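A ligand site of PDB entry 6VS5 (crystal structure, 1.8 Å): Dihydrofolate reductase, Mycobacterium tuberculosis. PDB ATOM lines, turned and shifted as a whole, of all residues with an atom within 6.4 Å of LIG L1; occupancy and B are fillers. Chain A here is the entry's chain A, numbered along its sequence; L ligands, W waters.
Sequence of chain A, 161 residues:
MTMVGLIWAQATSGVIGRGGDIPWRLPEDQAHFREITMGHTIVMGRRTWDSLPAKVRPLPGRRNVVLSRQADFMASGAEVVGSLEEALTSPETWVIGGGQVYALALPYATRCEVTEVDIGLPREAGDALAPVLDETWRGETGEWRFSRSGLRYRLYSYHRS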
ATOM      1  N   ALA A   9     -21.601 -29.723 -22.512  1.00  0.00           N
ATOM      2  CA  ALA A   9     -20.146 -29.766 -22.620  1.00  0.00           C
ATOM      3  C   ALA A   9     -19.617 -30.623 -21.481  1.00  0.00           C
ATOM      4  O   ALA A   9     -20.099 -30.523 -20.356  1.00  0.00           O
ATOM      5  CB  ALA A   9     -19.546 -28.353 -22.555  1.00  0.00           C
ATOM      6  N   ILE A  22     -19.615 -24.834 -13.448  1.00  0.00           N
ATOM      7  CA  ILE A  22     -18.829 -25.554 -14.460  1.00  0.00           C
ATOM      8  C   ILE A  22     -17.375 -25.230 -14.249  1.00  0.00           C
ATOM      9  O   ILE A  22     -17.013 -24.052 -14.124  1.00  0.00           O
ATOM     10  CB  ILE A  22     -19.271 -25.199 -15.892  1.00  0.00           C
ATOM     11  CG1 ILE A  22     -20.780 -25.411 -16.096  1.00  0.00           C
ATOM     12  CG2 ILE A  22     -18.459 -25.965 -16.906  1.00  0.00           C
ATOM     13  CD1 ILE A  22     -21.261 -24.906 -17.463  1.00  0.00           C
ATOM     14  N   TRP A  24     -14.919 -24.792 -16.095  1.00  0.00           N
ATOM     15  CA  TRP A  24     -14.268 -24.172 -17.249  1.00  0.00           C
ATOM     16  C   TRP A  24     -15.214 -23.113 -17.802  1.00  0.00           C
ATOM     17  O   TRP A  24     -16.353 -22.989 -17.363  1.00  0.00           O
ATOM     18  CB  TRP A  24     -13.903 -25.212 -18.312  1.00  0.00           C
ATOM     19  CG  TRP A  24     -15.092 -25.915 -18.903  1.00  0.00           C
ATOM     20  CD1 TRP A  24     -15.906 -25.462 -19.908  1.00  0.00           C
ATOM     21  CD2 TRP A  24     -15.591 -27.217 -18.536  1.00  0.00           C
ATOM     22  NE1 TRP A  24     -16.888 -26.390 -20.175  1.00  0.00           N
ATOM     23  CE2 TRP A  24     -16.711 -27.472 -19.352  1.00  0.00           C
ATOM     24  CE3 TRP A  24     -15.199 -28.175 -17.598  1.00  0.00           C
ATOM     25  CZ2 TRP A  24     -17.453 -28.652 -19.244  1.00  0.00           C
ATOM     26  CZ3 TRP A  24     -15.934 -29.346 -17.499  1.00  0.00           C
ATOM     27  CH2 TRP A  24     -17.044 -29.567 -18.309  1.00  0.00           C
ATOM     28  N   ARG A  25     -14.738 -22.374 -18.811  1.00  0.00           N
ATOM     29  CA  ARG A  25     -15.588 -21.418 -19.517  1.00  0.00           C
ATOM     30  C   ARG A  25     -15.032 -21.226 -20.920  1.00  0.00           C
ATOM     31  O   ARG A  25     -13.947 -20.669 -21.075  1.00  0.00           O
ATOM     32  CB  ARG A  25     -15.669 -20.086 -18.763  1.00  0.00           C
ATOM     33  CG  ARG A  25     -16.630 -19.080 -19.408  1.00  0.00           C
ATOM     34  CD  ARG A  25     -17.074 -17.986 -18.438  1.00  0.00           C
ATOM     35  NE  ARG A  25     -17.999 -18.502 -17.430  1.00  0.00           N
ATOM     36  CZ  ARG A  25     -18.633 -17.753 -16.530  1.00  0.00           C
ATOM     37  NH1 ARG A  25     -18.457 -16.440 -16.493  1.00  0.00           N
ATOM     38  NH2 ARG A  25     -19.449 -18.342 -15.651  1.00  0.00           N
ATOM     39  N   LEU A  26     -15.777 -21.710 -21.933  1.00  0.00           N
ATOM     40  CA  LEU A  26     -15.436 -21.512 -23.343  1.00  0.00           C
ATOM     41  C   LEU A  26     -16.386 -20.505 -23.958  1.00  0.00           C
ATOM     42  O   LEU A  26     -17.554 -20.827 -24.167  1.00  0.00           O
ATOM     43  CB  LEU A  26     -15.520 -22.832 -24.119  1.00  0.00           C
ATOM     44  CG  LEU A  26     -14.781 -24.064 -23.579  1.00  0.00           C
ATOM     45  CD1 LEU A  26     -15.023 -25.247 -24.506  1.00  0.00           C
ATOM     46  CD2 LEU A  26     -13.301 -23.794 -23.483  1.00  0.00           C
ATOM     47  N   PRO A  27     -15.943 -19.280 -24.273  1.00  0.00           N
ATOM     48  CA  PRO A  27     -16.859 -18.356 -24.968  1.00  0.00           C
ATOM     49  C   PRO A  27     -17.352 -18.914 -26.288  1.00  0.00           C
ATOM     50  O   PRO A  27     -18.522 -18.708 -26.650  1.00  0.00           O
ATOM     51  CB  PRO A  27     -15.992 -17.100 -25.157  1.00  0.00           C
ATOM     52  CG  PRO A  27     -14.947 -17.195 -24.095  1.00  0.00           C
ATOM     53  CD  PRO A  27     -14.654 -18.662 -23.934  1.00  0.00           C
ATOM     54  N   ASP A  29     -18.023 -22.018 -26.968  1.00  0.00           N
ATOM     55  CA  ASP A  29     -19.109 -22.955 -26.714  1.00  0.00           C
ATOM     56  C   ASP A  29     -20.377 -22.240 -26.278  1.00  0.00           C
ATOM     57  O   ASP A  29     -21.485 -22.723 -26.546  1.00  0.00           O
ATOM     58  CB  ASP A  29     -18.700 -23.973 -25.657  1.00  0.00           C
ATOM     59  CG  ASP A  29     -19.632 -25.168 -25.644  1.00  0.00           C
ATOM     60  OD1 ASP A  29     -19.960 -25.660 -26.743  1.00  0.00           O
ATOM     61  OD2 ASP A  29     -20.042 -25.603 -24.551  1.00  0.00           O
ATOM     62  N   GLN A  30     -20.245 -21.111 -25.586  1.00  0.00           N
ATOM     63  CA  GLN A  30     -21.420 -20.297 -25.263  1.00  0.00           C
ATOM     64  C   GLN A  30     -22.084 -19.799 -26.540  1.00  0.00           C
ATOM     65  O   GLN A  30     -23.321 -19.827 -26.664  1.00  0.00           O
ATOM     66  CB  GLN A  30     -21.026 -19.104 -24.390  1.00  0.00           C
ATOM     67  CG  GLN A  30     -20.570 -19.426 -22.984  1.00  0.00           C
ATOM     68  CD  GLN A  30     -20.320 -18.168 -22.156  1.00  0.00           C
ATOM     69  OE1 GLN A  30     -20.619 -17.048 -22.580  1.00  0.00           O
ATOM     70  NE2 GLN A  30     -19.751 -18.359 -20.962  1.00  0.00           N
ATOM     71  N   PHE A  33     -23.701 -22.733 -28.154  1.00  0.00           N
ATOM     72  CA  PHE A  33     -24.909 -23.003 -27.397  1.00  0.00           C
ATOM     73  C   PHE A  33     -26.021 -22.054 -27.780  1.00  0.00           C
ATOM     74  O   PHE A  33     -27.178 -22.469 -27.959  1.00  0.00           O
ATOM     75  CB  PHE A  33     -24.618 -22.886 -25.897  1.00  0.00           C
ATOM     76  CG  PHE A  33     -25.855 -22.926 -25.040  1.00  0.00           C
ATOM     77  CD1 PHE A  33     -26.432 -24.135 -24.667  1.00  0.00           C
ATOM     78  CD2 PHE A  33     -26.481 -21.744 -24.639  1.00  0.00           C
ATOM     79  CE1 PHE A  33     -27.564 -24.153 -23.898  1.00  0.00           C
ATOM     80  CE2 PHE A  33     -27.614 -21.776 -23.872  1.00  0.00           C
ATOM     81  CZ  PHE A  33     -28.149 -22.973 -23.512  1.00  0.00           C
ATOM     82  N   MET A  44     -34.437 -27.003 -18.396  1.00  0.00           N
ATOM     83  CA  MET A  44     -33.306 -27.125 -17.502  1.00  0.00           C
ATOM     84  C   MET A  44     -33.794 -27.520 -16.126  1.00  0.00           C
ATOM     85  O   MET A  44     -34.915 -27.180 -15.728  1.00  0.00           O
ATOM     86  CB  MET A  44     -32.512 -25.803 -17.434  1.00  0.00           C
ATOM     87  CG  MET A  44     -33.258 -24.669 -16.753  1.00  0.00           C
ATOM     88  SD  MET A  44     -32.517 -23.019 -16.902  1.00  0.00           S
ATOM     89  CE  MET A  44     -33.365 -22.429 -18.348  1.00  0.00           C
ATOM     90  N   THR A  48     -29.728 -25.976 -12.448  1.00  0.00           N
ATOM     91  CA  THR A  48     -29.108 -25.261 -13.558  1.00  0.00           C
ATOM     92  C   THR A  48     -29.639 -23.826 -13.660  1.00  0.00           C
ATOM     93  O   THR A  48     -28.854 -22.895 -13.853  1.00  0.00           O
ATOM     94  CB  THR A  48     -29.327 -26.039 -14.838  1.00  0.00           C
ATOM     95  OG1 THR A  48     -28.633 -27.293 -14.738  1.00  0.00           O
ATOM     96  CG2 THR A  48     -28.791 -25.264 -16.030  1.00  0.00           C
ATOM     97  N   SER A  51     -27.826 -21.802 -11.344  1.00  0.00           N
ATOM     98  CA  SER A  51     -26.471 -21.525 -11.829  1.00  0.00           C
ATOM     99  C   SER A  51     -26.433 -20.361 -12.811  1.00  0.00           C
ATOM    100  O   SER A  51     -25.350 -19.839 -13.085  1.00  0.00           O
ATOM    101  CB  SER A  51     -25.896 -22.767 -12.503  1.00  0.00           C
ATOM    102  OG  SER A  51     -26.385 -22.941 -13.830  1.00  0.00           O
ATOM    103  N   LEU A  52     -27.563 -19.941 -13.329  1.00  0.00           N
ATOM    104  CA  LEU A  52     -27.551 -18.826 -14.267  1.00  0.00           C
ATOM    105  C   LEU A  52     -27.447 -17.513 -13.504  1.00  0.00           C
ATOM    106  O   LEU A  52     -28.213 -17.294 -12.562  1.00  0.00           O
ATOM    107  CB  LEU A  52     -28.789 -18.841 -15.146  1.00  0.00           C
ATOM    108  CG  LEU A  52     -28.924 -20.006 -16.142  1.00  0.00           C
ATOM    109  CD1 LEU A  52     -30.219 -19.914 -16.953  1.00  0.00           C
ATOM    110  CD2 LEU A  52     -27.715 -20.130 -17.080  1.00  0.00           C
ATOM    111  N   LEU A  59     -32.644 -16.796 -20.409  1.00  0.00           N
ATOM    112  CA  LEU A  59     -31.819 -16.691 -21.601  1.00  0.00           C
ATOM    113  C   LEU A  59     -32.628 -16.062 -22.735  1.00  0.00           C
ATOM    114  O   LEU A  59     -33.728 -16.550 -23.056  1.00  0.00           O
ATOM    115  CB  LEU A  59     -31.292 -18.069 -21.990  1.00  0.00           C
ATOM    116  CG  LEU A  59     -30.340 -18.597 -20.922  1.00  0.00           C
ATOM    117  CD1 LEU A  59     -29.697 -19.892 -21.347  1.00  0.00           C
ATOM    118  CD2 LEU A  59     -29.276 -17.536 -20.637  1.00  0.00           C
ATOM    119  N   ILE A  96     -30.949 -28.391 -21.603  1.00  0.00           N
ATOM    120  CA  ILE A  96     -29.676 -27.692 -21.452  1.00  0.00           C
ATOM    121  C   ILE A  96     -28.973 -28.022 -20.124  1.00  0.00           C
ATOM    122  O   ILE A  96     -27.909 -27.459 -19.846  1.00  0.00           O
ATOM    123  CB  ILE A  96     -29.845 -26.170 -21.624  1.00  0.00           C
ATOM    124  CG1 ILE A  96     -30.633 -25.568 -20.481  1.00  0.00           C
ATOM    125  CG2 ILE A  96     -30.561 -25.858 -22.923  1.00  0.00           C
ATOM    126  CD1 ILE A  96     -30.537 -24.048 -20.466  1.00  0.00           C
ATOM    127  N   GLY A  97     -29.510 -28.953 -19.331  1.00  0.00           N
ATOM    128  CA  GLY A  97     -28.882 -29.391 -18.089  1.00  0.00           C
ATOM    129  C   GLY A  97     -29.812 -29.495 -16.887  1.00  0.00           C
ATOM    130  O   GLY A  97     -30.988 -29.159 -17.017  1.00  0.00           O
HETATM  131  C1  LIG L   1     -21.229 -23.767 -21.902  1.00  0.00           C
HETATM  132  C2  LIG L   1     -21.861 -21.238 -19.256  1.00  0.00           C
HETATM  133  C3  LIG L   1     -25.652 -23.262 -18.231  1.00  0.00           C
HETATM  134  C4  LIG L   1     -26.758 -23.315 -19.050  1.00  0.00           C
HETATM  135  C5  LIG L   1     -26.560 -23.292 -20.419  1.00  0.00           C
HETATM  136  C6  LIG L   1     -25.284 -23.229 -20.958  1.00  0.00           C
HETATM  137  C7  LIG L   1     -24.170 -23.154 -20.146  1.00  0.00           C
HETATM  138  C8  LIG L   1     -24.370 -23.206 -18.773  1.00  0.00           C
HETATM  139  N1  LIG L   1     -22.928 -23.115 -20.655  1.00  0.00           N
HETATM  140  C9  LIG L   1     -21.892 -22.351 -20.313  1.00  0.00           C
HETATM  141  C10 LIG L   1     -20.797 -22.724 -21.095  1.00  0.00           C
HETATM  142  N2  LIG L   1     -22.503 -23.984 -21.619  1.00  0.00           N
HETATM  143  C11 LIG L   1     -19.373 -22.178 -21.092  1.00  0.00           C
HETATM  144  O1  LIG L   1     -19.038 -21.147 -20.440  1.00  0.00           O
HETATM  145  O2  LIG L   1     -18.479 -22.806 -21.729  1.00  0.00           O
HETATM  146  C1  LG2 L   2     -25.800 -15.878 -22.131  1.00  0.00           C
HETATM  147  C2  LG2 L   2     -25.377 -19.554 -21.777  1.00  0.00           C
HETATM  148  C3  LG2 L   2     -22.194 -17.491 -18.273  1.00  0.00           C
HETATM  149  C4  LG2 L   2     -22.764 -18.375 -17.365  1.00  0.00           C
HETATM  150  C5  LG2 L   2     -24.019 -18.888 -17.594  1.00  0.00           C
HETATM  151  C6  LG2 L   2     -24.718 -18.514 -18.729  1.00  0.00           C
HETATM  152  C7  LG2 L   2     -24.145 -17.648 -19.661  1.00  0.00           C
HETATM  153  C8  LG2 L   2     -22.887 -17.125 -19.410  1.00  0.00           C
HETATM  154  N1  LG2 L   2     -24.837 -17.270 -20.744  1.00  0.00           N
HETATM  155  C9  LG2 L   2     -25.400 -18.023 -21.686  1.00  0.00           C
HETATM  156  C10 LG2 L   2     -26.024 -17.166 -22.589  1.00  0.00           C
HETATM  157  N2  LG2 L   2     -25.093 -15.964 -21.033  1.00  0.00           N
HETATM  158  C11 LG2 L   2     -26.822 -17.507 -23.835  1.00  0.00           C
HETATM  159  O1  LG2 L   2     -27.446 -16.579 -24.427  1.00  0.00           O
HETATM  160  O2  LG2 L   2     -26.911 -18.693 -24.245  1.00  0.00           O
HETATM  161  P1  LG3 L   3     -30.121 -30.149 -12.425  1.00  0.00           P
HETATM  162  O1  LG3 L   3     -30.306 -31.360 -13.271  1.00  0.00           O
HETATM  163  O2  LG3 L   3     -29.640 -28.858 -12.997  1.00  0.00           O
HETATM  164  O3  LG3 L   3     -31.576 -29.793 -11.723  1.00  0.00           O
HETATM  165  C1  LG3 L   3     -31.784 -30.729 -10.678  1.00  0.00           C
HETATM  166  C2  LG3 L   3     -33.184 -30.394 -10.160  1.00  0.00           C
HETATM  167  O4  LG3 L   3     -34.113 -30.627 -11.186  1.00  0.00           O
HETATM  168  C3  LG3 L   3     -33.642 -31.201  -8.951  1.00  0.00           C
HETATM  169  O5  LG3 L   3     -33.124 -30.678  -7.763  1.00  0.00           O
HETATM  170  C4  LG3 L   3     -35.170 -30.869  -9.035  1.00  0.00           C
HETATM  171  O6  LG3 L   3     -35.446 -29.610  -8.798  1.00  0.00           O
HETATM  172  C5  LG3 L   3     -35.365 -31.004 -10.558  1.00  0.00           C
HETATM  173  N1  LG3 L   3     -35.724 -32.368 -10.966  1.00  0.00           N
HETATM  174  C6  LG3 L   3     -34.887 -33.440 -11.214  1.00  0.00           C
HETATM  175  N2  LG3 L   3     -35.571 -34.577 -11.553  1.00  0.00           N
HETATM  176  C7  LG3 L   3     -36.916 -34.176 -11.520  1.00  0.00           C
HETATM  177  C8  LG3 L   3     -38.101 -34.863 -11.779  1.00  0.00           C
HETATM  178  N3  LG3 L   3     -38.096 -36.196 -12.147  1.00  0.00           N
HETATM  179  N4  LG3 L   3     -39.324 -34.255 -11.677  1.00  0.00           N
HETATM  180  C9  LG3 L   3     -39.280 -32.933 -11.316  1.00  0.00           C
HETATM  181  N5  LG3 L   3     -38.249 -32.143 -11.030  1.00  0.00           N
HETATM  182  C10 LG3 L   3     -37.039 -32.812 -11.144  1.00  0.00           C
HETATM  183  O7  LG3 L   3     -29.221 -30.649 -11.142  1.00  0.00           O
HETATM  184  P2  LG3 L   3     -27.753 -31.207 -11.434  1.00  0.00           P
HETATM  185  O8  LG3 L   3     -27.811 -32.557 -12.024  1.00  0.00           O
HETATM  186  O9  LG3 L   3     -26.927 -30.960 -10.200  1.00  0.00           O
HETATM  187  O10 LG3 L   3     -26.882 -30.348 -12.624  1.00  0.00           O
HETATM  188  C11 LG3 L   3     -26.420 -29.144 -12.146  1.00  0.00           C
HETATM  189  C12 LG3 L   3     -24.943 -29.017 -12.591  1.00  0.00           C
HETATM  190  O11 LG3 L   3     -24.836 -29.127 -14.048  1.00  0.00           O
HETATM  191  C13 LG3 L   3     -24.371 -27.609 -12.217  1.00  0.00           C
HETATM  192  O12 LG3 L   3     -23.056 -27.791 -11.784  1.00  0.00           O
HETATM  193  C14 LG3 L   3     -24.372 -26.898 -13.572  1.00  0.00           C
HETATM  194  O13 LG3 L   3     -23.384 -25.948 -13.690  1.00  0.00           O
HETATM  195  C15 LG3 L   3     -24.009 -28.101 -14.493  1.00  0.00           C
HETATM  196  N6  LG3 L   3     -24.332 -27.811 -15.909  1.00  0.00           N
HETATM  197  C16 LG3 L   3     -23.400 -28.115 -16.905  1.00  0.00           C
HETATM  198  C17 LG3 L   3     -23.642 -27.851 -18.221  1.00  0.00           C
HETATM  199  C18 LG3 L   3     -22.626 -28.209 -19.196  1.00  0.00           C
HETATM  200  O14 LG3 L   3     -22.828 -28.250 -20.413  1.00  0.00           O
HETATM  201  N7  LG3 L   3     -21.362 -28.533 -18.756  1.00  0.00           N
HETATM  202  C19 LG3 L   3     -24.908 -27.229 -18.675  1.00  0.00           C
HETATM  203  C20 LG3 L   3     -25.859 -26.990 -17.556  1.00  0.00           C
HETATM  204  C21 LG3 L   3     -25.564 -27.268 -16.268  1.00  0.00           C
HETATM  205  P3  LG3 L   3     -36.077 -29.215  -7.169  1.00  0.00           P
HETATM  206  O15 LG3 L   3     -34.852 -29.655  -6.440  1.00  0.00           O
HETATM  207  O16 LG3 L   3     -36.370 -27.710  -7.230  1.00  0.00           O
HETATM  208  O17 LG3 L   3     -37.262 -30.139  -7.169  1.00  0.00           O
HETATM  209  O   HOH W   1     -18.601 -21.443 -17.439  1.00  0.00           O
HETATM  210  O   HOH W   2     -18.189 -25.177 -22.516  1.00  0.00           O
HETATM  211  O   HOH W   3     -23.710 -26.404 -22.293  1.00  0.00           O
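O2 of LIG L1 sits at hydrogen-bond distance from N of Leu 26 (2.9 Å).
NE2 of Gln 30 lies within hydrogen-bond range of O1 of LIG L1, at 2.9 Å.
O2 of LG3 L3 lies within hydrogen-bond range of N of Thr 48, 2.9 Å away.
OG1 of Thr 48 is in hydrogen-bond range of O2 of LG3 L3, at 2.5 Å.
N of Ala 9 is in hydrogen-bond range of O14 of LG3 L3, at 2.8 Å.
The backbone carbonyl oxygen (O) of Ala 9 is in hydrogen-bond range of a nitrogen (N7) of LG3 L3 (2.8 Å).
Merely in contact with LIG L1: Ile 22, Arg 25, Asp 29, Phe 33 and Leu 52.
Hydrophobic or aromatic side chains that line LIG L1: Ile 22, Leu 26, Phe 33 and Leu 52.
Within 4 Å of LIG L1: Ile 22, Arg 25, Leu 26, Asp 29, Gln 30, Phe 33 and Leu 52.
Water W2 lies within hydrogen-bond range of an oxygen (O2) of LIG L1, the side-chain carboxylate (OD2) of Asp 29 and the indole nitrogen (NE1) of Trp 24.
Water W3 bridges O14 of LG3 L3 and N2 of LIG L1.
Water W1 lies within hydrogen-bond range of the backbone carbonyl oxygen (O) of Trp 24 (2.7 Å), the guanidinium group (NE) of Arg 25 (3.0 Å) and an oxygen (O1) of LIG L1 (3.0 Å).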
